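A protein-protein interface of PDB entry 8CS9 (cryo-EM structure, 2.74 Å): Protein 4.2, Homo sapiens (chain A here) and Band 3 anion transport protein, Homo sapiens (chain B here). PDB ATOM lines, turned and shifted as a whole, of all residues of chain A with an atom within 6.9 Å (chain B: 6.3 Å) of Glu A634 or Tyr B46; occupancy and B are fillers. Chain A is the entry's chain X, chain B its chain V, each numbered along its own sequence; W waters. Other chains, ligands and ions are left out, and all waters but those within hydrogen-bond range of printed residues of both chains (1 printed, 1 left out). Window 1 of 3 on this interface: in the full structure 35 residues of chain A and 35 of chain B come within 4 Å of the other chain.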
ATOM      1  N   ASP A 180      31.659  -0.720  18.659  1.00  0.00           N
ATOM      2  CA  ASP A 180      32.892  -0.017  18.322  1.00  0.00           C
ATOM      3  C   ASP A 180      33.137   1.025  19.406  1.00  0.00           C
ATOM      4  O   ASP A 180      32.535   2.099  19.396  1.00  0.00           O
ATOM      5  CB  ASP A 180      32.796   0.619  16.940  1.00  0.00           C
ATOM      6  CG  ASP A 180      34.038   1.402  16.571  1.00  0.00           C
ATOM      7  OD1 ASP A 180      35.140   1.030  17.021  1.00  0.00           O
ATOM      8  OD2 ASP A 180      33.913   2.399  15.833  1.00  0.00           O
ATOM      9  N   GLU A 185      39.914   7.089  18.301  1.00  0.00           N
ATOM     10  CA  GLU A 185      39.527   8.068  17.301  1.00  0.00           C
ATOM     11  C   GLU A 185      40.190   9.408  17.610  1.00  0.00           C
ATOM     12  O   GLU A 185      40.543   9.708  18.754  1.00  0.00           O
ATOM     13  CB  GLU A 185      38.008   8.219  17.257  1.00  0.00           C
ATOM     14  CG  GLU A 185      37.333   7.498  16.110  1.00  0.00           C
ATOM     15  CD  GLU A 185      37.308   8.319  14.836  1.00  0.00           C
ATOM     16  OE1 GLU A 185      36.398   9.162  14.690  1.00  0.00           O
ATOM     17  OE2 GLU A 185      38.192   8.117  13.977  1.00  0.00           O
ATOM     18  N   LYS A 244      19.448   2.644  15.457  1.00  0.00           N
ATOM     19  CA  LYS A 244      20.671   2.318  14.737  1.00  0.00           C
ATOM     20  C   LYS A 244      21.869   2.921  15.460  1.00  0.00           C
ATOM     21  O   LYS A 244      21.898   4.125  15.733  1.00  0.00           O
ATOM     22  CB  LYS A 244      20.597   2.832  13.301  1.00  0.00           C
ATOM     23  CG  LYS A 244      21.499   2.102  12.331  1.00  0.00           C
ATOM     24  CD  LYS A 244      21.393   2.685  10.934  1.00  0.00           C
ATOM     25  CE  LYS A 244      20.242   2.064  10.164  1.00  0.00           C
ATOM     26  NZ  LYS A 244      20.452   0.615   9.933  1.00  0.00           N
ATOM     27  N   ARG A 245      22.858   2.088  15.762  1.00  0.00           N
ATOM     28  CA  ARG A 245      24.010   2.499  16.547  1.00  0.00           C
ATOM     29  C   ARG A 245      25.297   2.240  15.780  1.00  0.00           C
ATOM     30  O   ARG A 245      25.415   1.260  15.040  1.00  0.00           O
ATOM     31  CB  ARG A 245      24.051   1.770  17.895  1.00  0.00           C
ATOM     32  CG  ARG A 245      22.865   2.064  18.793  1.00  0.00           C
ATOM     33  CD  ARG A 245      23.136   3.237  19.723  1.00  0.00           C
ATOM     34  NE  ARG A 245      23.252   4.502  19.008  1.00  0.00           N
ATOM     35  CZ  ARG A 245      22.225   5.256  18.643  1.00  0.00           C
ATOM     36  NH1 ARG A 245      20.979   4.907  18.914  1.00  0.00           N
ATOM     37  NH2 ARG A 245      22.454   6.391  17.991  1.00  0.00           N
ATOM     38  N   ARG A 246      26.265   3.135  15.966  1.00  0.00           N
ATOM     39  CA  ARG A 246      27.568   3.038  15.321  1.00  0.00           C
ATOM     40  C   ARG A 246      28.686   3.202  16.339  1.00  0.00           C
ATOM     41  O   ARG A 246      29.745   3.760  16.044  1.00  0.00           O
ATOM     42  CB  ARG A 246      27.698   4.062  14.198  1.00  0.00           C
ATOM     43  CG  ARG A 246      26.811   3.768  13.006  1.00  0.00           C
ATOM     44  CD  ARG A 246      27.178   2.445  12.368  1.00  0.00           C
ATOM     45  NE  ARG A 246      26.468   2.224  11.115  1.00  0.00           N
ATOM     46  CZ  ARG A 246      25.442   1.396  10.973  1.00  0.00           C
ATOM     47  NH1 ARG A 246      24.974   0.695  11.991  1.00  0.00           N
ATOM     48  NH2 ARG A 246      24.871   1.269   9.780  1.00  0.00           N
ATOM     49  N   PRO A 250      30.097   8.362  18.111  1.00  0.00           N
ATOM     50  CA  PRO A 250      29.012   9.288  17.737  1.00  0.00           C
ATOM     51  C   PRO A 250      28.136   9.702  18.904  1.00  0.00           C
ATOM     52  O   PRO A 250      27.696  10.857  18.955  1.00  0.00           O
ATOM     53  CB  PRO A 250      28.218   8.495  16.690  1.00  0.00           C
ATOM     54  CG  PRO A 250      29.164   7.516  16.158  1.00  0.00           C
ATOM     55  CD  PRO A 250      30.059   7.141  17.282  1.00  0.00           C
ATOM     56  N   ARG A 253      30.080  12.345  20.771  1.00  0.00           N
ATOM     57  CA  ARG A 253      30.065  13.592  20.015  1.00  0.00           C
ATOM     58  C   ARG A 253      28.729  14.306  20.153  1.00  0.00           C
ATOM     59  O   ARG A 253      28.689  15.525  20.345  1.00  0.00           O
ATOM     60  CB  ARG A 253      30.369  13.325  18.542  1.00  0.00           C
ATOM     61  CG  ARG A 253      31.816  12.992  18.240  1.00  0.00           C
ATOM     62  CD  ARG A 253      31.977  12.584  16.789  1.00  0.00           C
ATOM     63  NE  ARG A 253      33.351  12.230  16.460  1.00  0.00           N
ATOM     64  CZ  ARG A 253      33.690  11.361  15.520  1.00  0.00           C
ATOM     65  NH1 ARG A 253      32.779  10.747  14.786  1.00  0.00           N
ATOM     66  NH2 ARG A 253      34.976  11.100  15.311  1.00  0.00           N
ATOM     67  N   ILE A 623      21.407  -3.913   3.328  1.00  0.00           N
ATOM     68  CA  ILE A 623      22.501  -4.533   4.065  1.00  0.00           C
ATOM     69  C   ILE A 623      23.672  -3.561   4.095  1.00  0.00           C
ATOM     70  O   ILE A 623      24.003  -2.942   3.077  1.00  0.00           O
ATOM     71  CB  ILE A 623      22.906  -5.887   3.453  1.00  0.00           C
ATOM     72  CG1 ILE A 623      24.097  -6.476   4.208  1.00  0.00           C
ATOM     73  CG2 ILE A 623      23.214  -5.759   1.967  1.00  0.00           C
ATOM     74  CD1 ILE A 623      24.331  -7.921   3.929  1.00  0.00           C
ATOM     75  N   SER A 624      24.276  -3.401   5.269  1.00  0.00           N
ATOM     76  CA  SER A 624      25.428  -2.533   5.443  1.00  0.00           C
ATOM     77  C   SER A 624      26.605  -3.335   5.978  1.00  0.00           C
ATOM     78  O   SER A 624      26.437  -4.253   6.785  1.00  0.00           O
ATOM     79  CB  SER A 624      25.118  -1.371   6.396  1.00  0.00           C
ATOM     80  OG  SER A 624      23.916  -0.719   6.041  1.00  0.00           O
ATOM     81  N   ILE A 625      27.799  -2.983   5.516  1.00  0.00           N
ATOM     82  CA  ILE A 625      29.036  -3.588   5.988  1.00  0.00           C
ATOM     83  C   ILE A 625      29.972  -2.478   6.443  1.00  0.00           C
ATOM     84  O   ILE A 625      30.056  -1.421   5.809  1.00  0.00           O
ATOM     85  CB  ILE A 625      29.706  -4.466   4.906  1.00  0.00           C
ATOM     86  CG1 ILE A 625      29.936  -3.676   3.618  1.00  0.00           C
ATOM     87  CG2 ILE A 625      28.868  -5.699   4.625  1.00  0.00           C
ATOM     88  CD1 ILE A 625      30.850  -4.367   2.646  1.00  0.00           C
ATOM     89  N   LEU A 626      30.658  -2.709   7.557  1.00  0.00           N
ATOM     90  CA  LEU A 626      31.629  -1.759   8.073  1.00  0.00           C
ATOM     91  C   LEU A 626      32.675  -2.518   8.876  1.00  0.00           C
ATOM     92  O   LEU A 626      32.678  -3.750   8.930  1.00  0.00           O
ATOM     93  CB  LEU A 626      30.957  -0.668   8.915  1.00  0.00           C
ATOM     94  CG  LEU A 626      30.030  -1.065  10.066  1.00  0.00           C
ATOM     95  CD1 LEU A 626      30.787  -1.217  11.376  1.00  0.00           C
ATOM     96  CD2 LEU A 626      28.925  -0.039  10.212  1.00  0.00           C
ATOM     97  N   GLY A 627      33.563  -1.763   9.510  1.00  0.00           N
ATOM     98  CA  GLY A 627      34.614  -2.325  10.327  1.00  0.00           C
ATOM     99  C   GLY A 627      35.886  -1.515  10.228  1.00  0.00           C
ATOM    100  O   GLY A 627      36.374  -1.243   9.130  1.00  0.00           O
ATOM    101  N   ILE A 631      37.035  -1.359   6.062  1.00  0.00           N
ATOM    102  CA  ILE A 631      36.123  -0.576   5.241  1.00  0.00           C
ATOM    103  C   ILE A 631      36.118   0.853   5.764  1.00  0.00           C
ATOM    104  O   ILE A 631      35.984   1.073   6.972  1.00  0.00           O
ATOM    105  CB  ILE A 631      34.702  -1.175   5.256  1.00  0.00           C
ATOM    106  CG1 ILE A 631      34.694  -2.519   4.527  1.00  0.00           C
ATOM    107  CG2 ILE A 631      33.696  -0.224   4.631  1.00  0.00           C
ATOM    108  CD1 ILE A 631      33.575  -3.421   4.932  1.00  0.00           C
ATOM    109  N   HIS A 632      36.275   1.816   4.861  1.00  0.00           N
ATOM    110  CA  HIS A 632      36.186   3.220   5.236  1.00  0.00           C
ATOM    111  C   HIS A 632      34.728   3.592   5.459  1.00  0.00           C
ATOM    112  O   HIS A 632      33.926   3.559   4.520  1.00  0.00           O
ATOM    113  CB  HIS A 632      36.811   4.100   4.158  1.00  0.00           C
ATOM    114  CG  HIS A 632      36.594   5.565   4.375  1.00  0.00           C
ATOM    115  ND1 HIS A 632      37.319   6.297   5.288  1.00  0.00           N
ATOM    116  CD2 HIS A 632      35.724   6.430   3.806  1.00  0.00           C
ATOM    117  CE1 HIS A 632      36.910   7.552   5.265  1.00  0.00           C
ATOM    118  NE2 HIS A 632      35.942   7.659   4.375  1.00  0.00           N
ATOM    119  N   ARG A 633      34.393   3.950   6.699  1.00  0.00           N
ATOM    120  CA  ARG A 633      33.024   4.248   7.135  1.00  0.00           C
ATOM    121  C   ARG A 633      32.165   3.024   6.840  1.00  0.00           C
ATOM    122  O   ARG A 633      32.553   1.913   7.242  1.00  0.00           O
ATOM    123  CB  ARG A 633      32.565   5.564   6.507  1.00  0.00           C
ATOM    124  CG  ARG A 633      33.531   6.707   6.730  1.00  0.00           C
ATOM    125  CD  ARG A 633      32.928   8.039   6.347  1.00  0.00           C
ATOM    126  NE  ARG A 633      33.713   9.151   6.866  1.00  0.00           N
ATOM    127  CZ  ARG A 633      33.334  10.419   6.829  1.00  0.00           C
ATOM    128  NH1 ARG A 633      32.174  10.778   6.308  1.00  0.00           N
ATOM    129  NH2 ARG A 633      34.139  11.351   7.330  1.00  0.00           N
ATOM    130  N   GLU A 634      31.026   3.151   6.167  1.00  0.00           N
ATOM    131  CA  GLU A 634      30.210   1.985   5.868  1.00  0.00           C
ATOM    132  C   GLU A 634      29.709   2.063   4.434  1.00  0.00           C
ATOM    133  O   GLU A 634      29.609   3.144   3.852  1.00  0.00           O
ATOM    134  CB  GLU A 634      29.029   1.857   6.833  1.00  0.00           C
ATOM    135  CG  GLU A 634      28.106   3.050   6.852  1.00  0.00           C
ATOM    136  CD  GLU A 634      26.795   2.747   7.534  1.00  0.00           C
ATOM    137  OE1 GLU A 634      25.998   1.966   6.972  1.00  0.00           O
ATOM    138  OE2 GLU A 634      26.558   3.283   8.634  1.00  0.00           O
ATOM    139  N   ARG A 635      29.401   0.895   3.876  1.00  0.00           N
ATOM    140  CA  ARG A 635      28.839   0.767   2.536  1.00  0.00           C
ATOM    141  C   ARG A 635      27.515   0.026   2.657  1.00  0.00           C
ATOM    142  O   ARG A 635      27.486  -1.128   3.094  1.00  0.00           O
ATOM    143  CB  ARG A 635      29.798   0.022   1.608  1.00  0.00           C
ATOM    144  CG  ARG A 635      30.888   0.879   1.005  1.00  0.00           C
ATOM    145  CD  ARG A 635      31.650   0.123  -0.061  1.00  0.00           C
ATOM    146  NE  ARG A 635      32.981  -0.274   0.378  1.00  0.00           N
ATOM    147  CZ  ARG A 635      33.396  -1.528   0.468  1.00  0.00           C
ATOM    148  NH1 ARG A 635      32.603  -2.543   0.167  1.00  0.00           N
ATOM    149  NH2 ARG A 635      34.640  -1.774   0.866  1.00  0.00           N
ATOM    150  N   SER A 636      26.427   0.677   2.267  1.00  0.00           N
ATOM    151  CA  SER A 636      25.102   0.079   2.312  1.00  0.00           C
ATOM    152  C   SER A 636      24.674  -0.356   0.918  1.00  0.00           C
ATOM    153  O   SER A 636      24.881   0.367  -0.061  1.00  0.00           O
ATOM    154  CB  SER A 636      24.077   1.053   2.894  1.00  0.00           C
ATOM    155  OG  SER A 636      24.559   1.646   4.084  1.00  0.00           O
ATOM    156  N   TYR A 637      24.082  -1.542   0.834  1.00  0.00           N
ATOM    157  CA  TYR A 637      23.626  -2.105  -0.426  1.00  0.00           C
ATOM    158  C   TYR A 637      22.177  -2.549  -0.296  1.00  0.00           C
ATOM    159  O   TYR A 637      21.683  -2.816   0.800  1.00  0.00           O
ATOM    160  CB  TYR A 637      24.478  -3.306  -0.876  1.00  0.00           C
ATOM    161  CG  TYR A 637      25.979  -3.092  -0.921  1.00  0.00           C
ATOM    162  CD1 TYR A 637      26.736  -3.037   0.242  1.00  0.00           C
ATOM    163  CD2 TYR A 637      26.641  -2.983  -2.134  1.00  0.00           C
ATOM    164  CE1 TYR A 637      28.100  -2.857   0.197  1.00  0.00           C
ATOM    165  CE2 TYR A 637      28.004  -2.803  -2.186  1.00  0.00           C
ATOM    166  CZ  TYR A 637      28.729  -2.741  -1.018  1.00  0.00           C
ATOM    167  OH  TYR A 637      30.089  -2.563  -1.071  1.00  0.00           O
ATOM    168  N   GLU A 667      25.122  -5.494   8.982  1.00  0.00           N
ATOM    169  CA  GLU A 667      23.809  -5.098   9.468  1.00  0.00           C
ATOM    170  C   GLU A 667      22.791  -5.263   8.351  1.00  0.00           C
ATOM    171  O   GLU A 667      23.020  -4.814   7.226  1.00  0.00           O
ATOM    172  CB  GLU A 667      23.818  -3.649   9.965  1.00  0.00           C
ATOM    173  CG  GLU A 667      22.653  -3.294  10.866  1.00  0.00           C
ATOM    174  CD  GLU A 667      22.390  -1.805  10.910  1.00  0.00           C
ATOM    175  OE1 GLU A 667      21.872  -1.261   9.912  1.00  0.00           O
ATOM    176  OE2 GLU A 667      22.697  -1.176  11.945  1.00  0.00           O
ATOM    177  N   THR B  42      23.543   7.459   8.486  1.00  0.00           N
ATOM    178  CA  THR B  42      24.642   7.450   9.443  1.00  0.00           C
ATOM    179  C   THR B  42      25.839   8.258   8.955  1.00  0.00           C
ATOM    180  O   THR B  42      26.965   8.017   9.400  1.00  0.00           O
ATOM    181  CB  THR B  42      25.066   6.014   9.750  1.00  0.00           C
ATOM    182  OG1 THR B  42      25.387   5.336   8.531  1.00  0.00           O
ATOM    183  CG2 THR B  42      23.948   5.269  10.452  1.00  0.00           C
ATOM    184  N   ALA B  43      25.619   9.203   8.038  1.00  0.00           N
ATOM    185  CA  ALA B  43      26.715  10.033   7.550  1.00  0.00           C
ATOM    186  C   ALA B  43      27.275  10.920   8.653  1.00  0.00           C
ATOM    187  O   ALA B  43      28.494  11.083   8.767  1.00  0.00           O
ATOM    188  CB  ALA B  43      26.247  10.877   6.366  1.00  0.00           C
ATOM    189  N   THR B  44      26.400  11.494   9.482  1.00  0.00           N
ATOM    190  CA  THR B  44      26.845  12.356  10.570  1.00  0.00           C
ATOM    191  C   THR B  44      27.574  11.594  11.669  1.00  0.00           C
ATOM    192  O   THR B  44      28.233  12.225  12.501  1.00  0.00           O
ATOM    193  CB  THR B  44      25.657  13.107  11.174  1.00  0.00           C
ATOM    194  OG1 THR B  44      26.075  13.776  12.369  1.00  0.00           O
ATOM    195  CG2 THR B  44      24.530  12.145  11.507  1.00  0.00           C
ATOM    196  N   ASP B  45      27.478  10.264  11.691  1.00  0.00           N
ATOM    197  CA  ASP B  45      28.170   9.461  12.690  1.00  0.00           C
ATOM    198  C   ASP B  45      29.677   9.428  12.480  1.00  0.00           C
ATOM    199  O   ASP B  45      30.394   8.927  13.350  1.00  0.00           O
ATOM    200  CB  ASP B  45      27.620   8.035  12.686  1.00  0.00           C
ATOM    201  CG  ASP B  45      26.295   7.922  13.406  1.00  0.00           C
ATOM    202  OD1 ASP B  45      25.685   8.969  13.695  1.00  0.00           O
ATOM    203  OD2 ASP B  45      25.862   6.788  13.691  1.00  0.00           O
ATOM    204  N   TYR B  46      30.171   9.941  11.353  1.00  0.00           N
ATOM    205  CA  TYR B  46      31.598   9.969  11.059  1.00  0.00           C
ATOM    206  C   TYR B  46      32.131  11.393  10.947  1.00  0.00           C
ATOM    207  O   TYR B  46      33.253  11.595  10.476  1.00  0.00           O
ATOM    208  CB  TYR B  46      31.889   9.186   9.780  1.00  0.00           C
ATOM    209  CG  TYR B  46      31.369   7.770   9.807  1.00  0.00           C
ATOM    210  CD1 TYR B  46      32.105   6.752  10.396  1.00  0.00           C
ATOM    211  CD2 TYR B  46      30.140   7.450   9.249  1.00  0.00           C
ATOM    212  CE1 TYR B  46      31.635   5.457  10.425  1.00  0.00           C
ATOM    213  CE2 TYR B  46      29.659   6.156   9.275  1.00  0.00           C
ATOM    214  CZ  TYR B  46      30.411   5.164   9.863  1.00  0.00           C
ATOM    215  OH  TYR B  46      29.940   3.874   9.892  1.00  0.00           O
ATOM    216  N   HIS B  47      31.353  12.382  11.376  1.00  0.00           N
ATOM    217  CA  HIS B  47      31.776  13.778  11.354  1.00  0.00           C
ATOM    218  C   HIS B  47      32.550  14.071  12.633  1.00  0.00           C
ATOM    219  O   HIS B  47      31.968  14.119  13.721  1.00  0.00           O
ATOM    220  CB  HIS B  47      30.573  14.707  11.215  1.00  0.00           C
ATOM    221  CG  HIS B  47      29.877  14.602   9.896  1.00  0.00           C
ATOM    222  ND1 HIS B  47      28.745  15.327   9.594  1.00  0.00           N
ATOM    223  CD2 HIS B  47      30.150  13.857   8.799  1.00  0.00           C
ATOM    224  CE1 HIS B  47      28.352  15.034   8.368  1.00  0.00           C
ATOM    225  NE2 HIS B  47      29.186  14.145   7.864  1.00  0.00           N
ATOM    226  N   THR B  48      33.857  14.268  12.505  1.00  0.00           N
ATOM    227  CA  THR B  48      34.695  14.506  13.669  1.00  0.00           C
ATOM    228  C   THR B  48      34.460  15.903  14.234  1.00  0.00           C
ATOM    229  O   THR B  48      34.066  16.831  13.523  1.00  0.00           O
ATOM    230  CB  THR B  48      36.171  14.330  13.317  1.00  0.00           C
ATOM    231  OG1 THR B  48      36.978  14.735  14.428  1.00  0.00           O
ATOM    232  CG2 THR B  48      36.535  15.171  12.105  1.00  0.00           C
ATOM    233  N   LEU B 121      36.830  11.237   2.776  1.00  0.00           N
ATOM    234  CA  LEU B 121      37.183  12.310   3.695  1.00  0.00           C
ATOM    235  C   LEU B 121      37.556  11.721   5.046  1.00  0.00           C
ATOM    236  O   LEU B 121      36.855  10.841   5.557  1.00  0.00           O
ATOM    237  CB  LEU B 121      36.023  13.297   3.833  1.00  0.00           C
ATOM    238  CG  LEU B 121      35.622  14.025   2.547  1.00  0.00           C
ATOM    239  CD1 LEU B 121      34.810  15.256   2.862  1.00  0.00           C
ATOM    240  CD2 LEU B 121      36.840  14.402   1.724  1.00  0.00           C
ATOM    241  N   ASP B 122      38.660  12.214   5.614  1.00  0.00           N
ATOM    242  CA  ASP B 122      39.247  11.680   6.845  1.00  0.00           C
ATOM    243  C   ASP B 122      39.545  10.189   6.704  1.00  0.00           C
ATOM    244  O   ASP B 122      39.135   9.365   7.523  1.00  0.00           O
ATOM    245  CB  ASP B 122      38.355  11.958   8.058  1.00  0.00           C
ATOM    246  CG  ASP B 122      38.172  13.437   8.317  1.00  0.00           C
ATOM    247  OD1 ASP B 122      39.171  14.182   8.252  1.00  0.00           O
ATOM    248  OD2 ASP B 122      37.027  13.859   8.584  1.00  0.00           O
ATOM    249  N   ARG B 138      35.760   2.418  -3.278  1.00  0.00           N
ATOM    250  CA  ARG B 138      34.700   3.421  -3.332  1.00  0.00           C
ATOM    251  C   ARG B 138      34.336   3.790  -4.769  1.00  0.00           C
ATOM    252  O   ARG B 138      33.191   4.164  -5.035  1.00  0.00           O
ATOM    253  CB  ARG B 138      35.113   4.661  -2.544  1.00  0.00           C
ATOM    254  CG  ARG B 138      33.946   5.468  -2.019  1.00  0.00           C
ATOM    255  CD  ARG B 138      33.282   4.780  -0.847  1.00  0.00           C
ATOM    256  NE  ARG B 138      31.953   5.315  -0.580  1.00  0.00           N
ATOM    257  CZ  ARG B 138      31.213   4.985   0.468  1.00  0.00           C
ATOM    258  NH1 ARG B 138      31.649   4.135   1.383  1.00  0.00           N
ATOM    259  NH2 ARG B 138      30.005   5.524   0.605  1.00  0.00           N
ATOM    260  N   PHE B 141      31.990   1.104  -5.659  1.00  0.00           N
ATOM    261  CA  PHE B 141      30.736   1.273  -4.932  1.00  0.00           C
ATOM    262  C   PHE B 141      29.843   2.318  -5.588  1.00  0.00           C
ATOM    263  O   PHE B 141      28.626   2.132  -5.686  1.00  0.00           O
ATOM    264  CB  PHE B 141      31.020   1.649  -3.479  1.00  0.00           C
ATOM    265  CG  PHE B 141      29.790   1.743  -2.627  1.00  0.00           C
ATOM    266  CD1 PHE B 141      28.993   0.633  -2.407  1.00  0.00           C
ATOM    267  CD2 PHE B 141      29.426   2.944  -2.048  1.00  0.00           C
ATOM    268  CE1 PHE B 141      27.862   0.719  -1.628  1.00  0.00           C
ATOM    269  CE2 PHE B 141      28.295   3.034  -1.268  1.00  0.00           C
ATOM    270  CZ  PHE B 141      27.511   1.920  -1.059  1.00  0.00           C
ATOM    271  N   GLN B 302      32.850  17.748   4.977  1.00  0.00           N
ATOM    272  CA  GLN B 302      32.395  16.445   5.436  1.00  0.00           C
ATOM    273  C   GLN B 302      31.687  15.642   4.358  1.00  0.00           C
ATOM    274  O   GLN B 302      31.545  14.424   4.510  1.00  0.00           O
ATOM    275  CB  GLN B 302      31.465  16.594   6.647  1.00  0.00           C
ATOM    276  CG  GLN B 302      32.190  16.818   7.960  1.00  0.00           C
ATOM    277  CD  GLN B 302      33.355  15.865   8.161  1.00  0.00           C
ATOM    278  OE1 GLN B 302      33.208  14.650   8.041  1.00  0.00           O
ATOM    279  NE2 GLN B 302      34.522  16.415   8.466  1.00  0.00           N
HETATM  280  O   HOH W   1      33.805   9.844   3.077  1.00  0.00           O
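Of chain B, only Thr B42 (2.4 Å), Tyr B46 (3.6 Å) and Arg B138 (3.4 Å) come within 4 Å of Glu A634. Tyr B46 touches just these residues of chain A: Arg A246 (3.98 Å), Arg A253 (3.9 Å), Arg A633 (3.3 Å) and Glu A634 (3.6 Å). Of the printed residues of chain A, Thr B42 touches Lys A244 and Glu A634. Of the printed residues of chain A, Thr B48 touches Arg A253 (3.8 Å). Printed residues of chain B within 4 Å of Arg A633: Tyr B46 (3.3 Å), Leu B121 (3.3 Å) and Gln B302 (3.5 Å). Gly A627 touches none of the printed residues of chain B. The nearest residue of chain B that does not touch Glu A634 is Phe B141 (5.3 Å). The nearest residue of chain A that does not touch Tyr B46 is Leu A626 (4.1 Å).
Of the 20 printed residues of chain A, 10 touch a printed residue of chain B. Of the 12 printed residues of chain B, 10 touch a printed residue of chain A. Hydrophobic or aromatic side chains of chain B within 4 Å of the printed part of chain A: Tyr B46 and Phe B141.
Thr B42 touches Lys A244 (CG2 to CD, 3.7 Å). CG of Arg A246 touches OD2 of Asp B45, at 3.2 Å. Asp B45 touches Pro A250 (O to CG, 3.4 Å). His B47 touches Arg A253. Leu B121 touches His A632 (O to CE1, 3.3 Å). His A632 touches Asp B122. Tyr B46 touches Glu A634 (OH to CG, 3.6 Å). Arg B138 touches Arg A635. Arg A635 touches Phe B141. O of Ser A636 touches CZ of Phe B141, at 3.2 Å.
OG of Ser A624 lies within hydrogen-bond range of OG of Ser A636, 3.1 Å away. The backbone NH of Tyr A637 is in hydrogen-bond range of the backbone carbonyl oxygen of Ile A623, 2.6 Å away. The side-chain amino group (NZ) of Lys A244 is in salt-bridge range of the side-chain carboxylate (OE2) of Glu A667. NH1 of Arg A635 sits at hydrogen-bond distance from OH of Tyr A637. OG of Ser A636 is in hydrogen-bond range of OE1 of Glu A634. The backbone NH (N) of Ile A625 sits at hydrogen-bond distance from the backbone carbonyl oxygen (O) of Arg A635 (3.1 Å).
Water W1 bridges NE2 of His A632 (3.3 Å) and N of Leu B121 (3.3 Å).
The backbone carbonyl oxygen (O) of Leu B121 lies within hydrogen-bond range of the guanidinium group (NH2) of Arg A633 (3.3 Å). The side-chain carboxylate (OE2) of Glu A634 lies close to the side-chain hydroxyl (OG1) of Thr B42, at 2.4 Å. The backbone carbonyl oxygen of Asp B45 is in hydrogen-bond range of the guanidinium group of Arg A253, at 3.3 Å. The backbone carbonyl oxygen of Glu A634 is in hydrogen-bond range of the guanidinium group of Arg B138. The guanidinium group (NH2) of Arg A633 sits at hydrogen-bond distance from the backbone carbonyl oxygen (O) of Tyr B46, at 3.3 Å.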
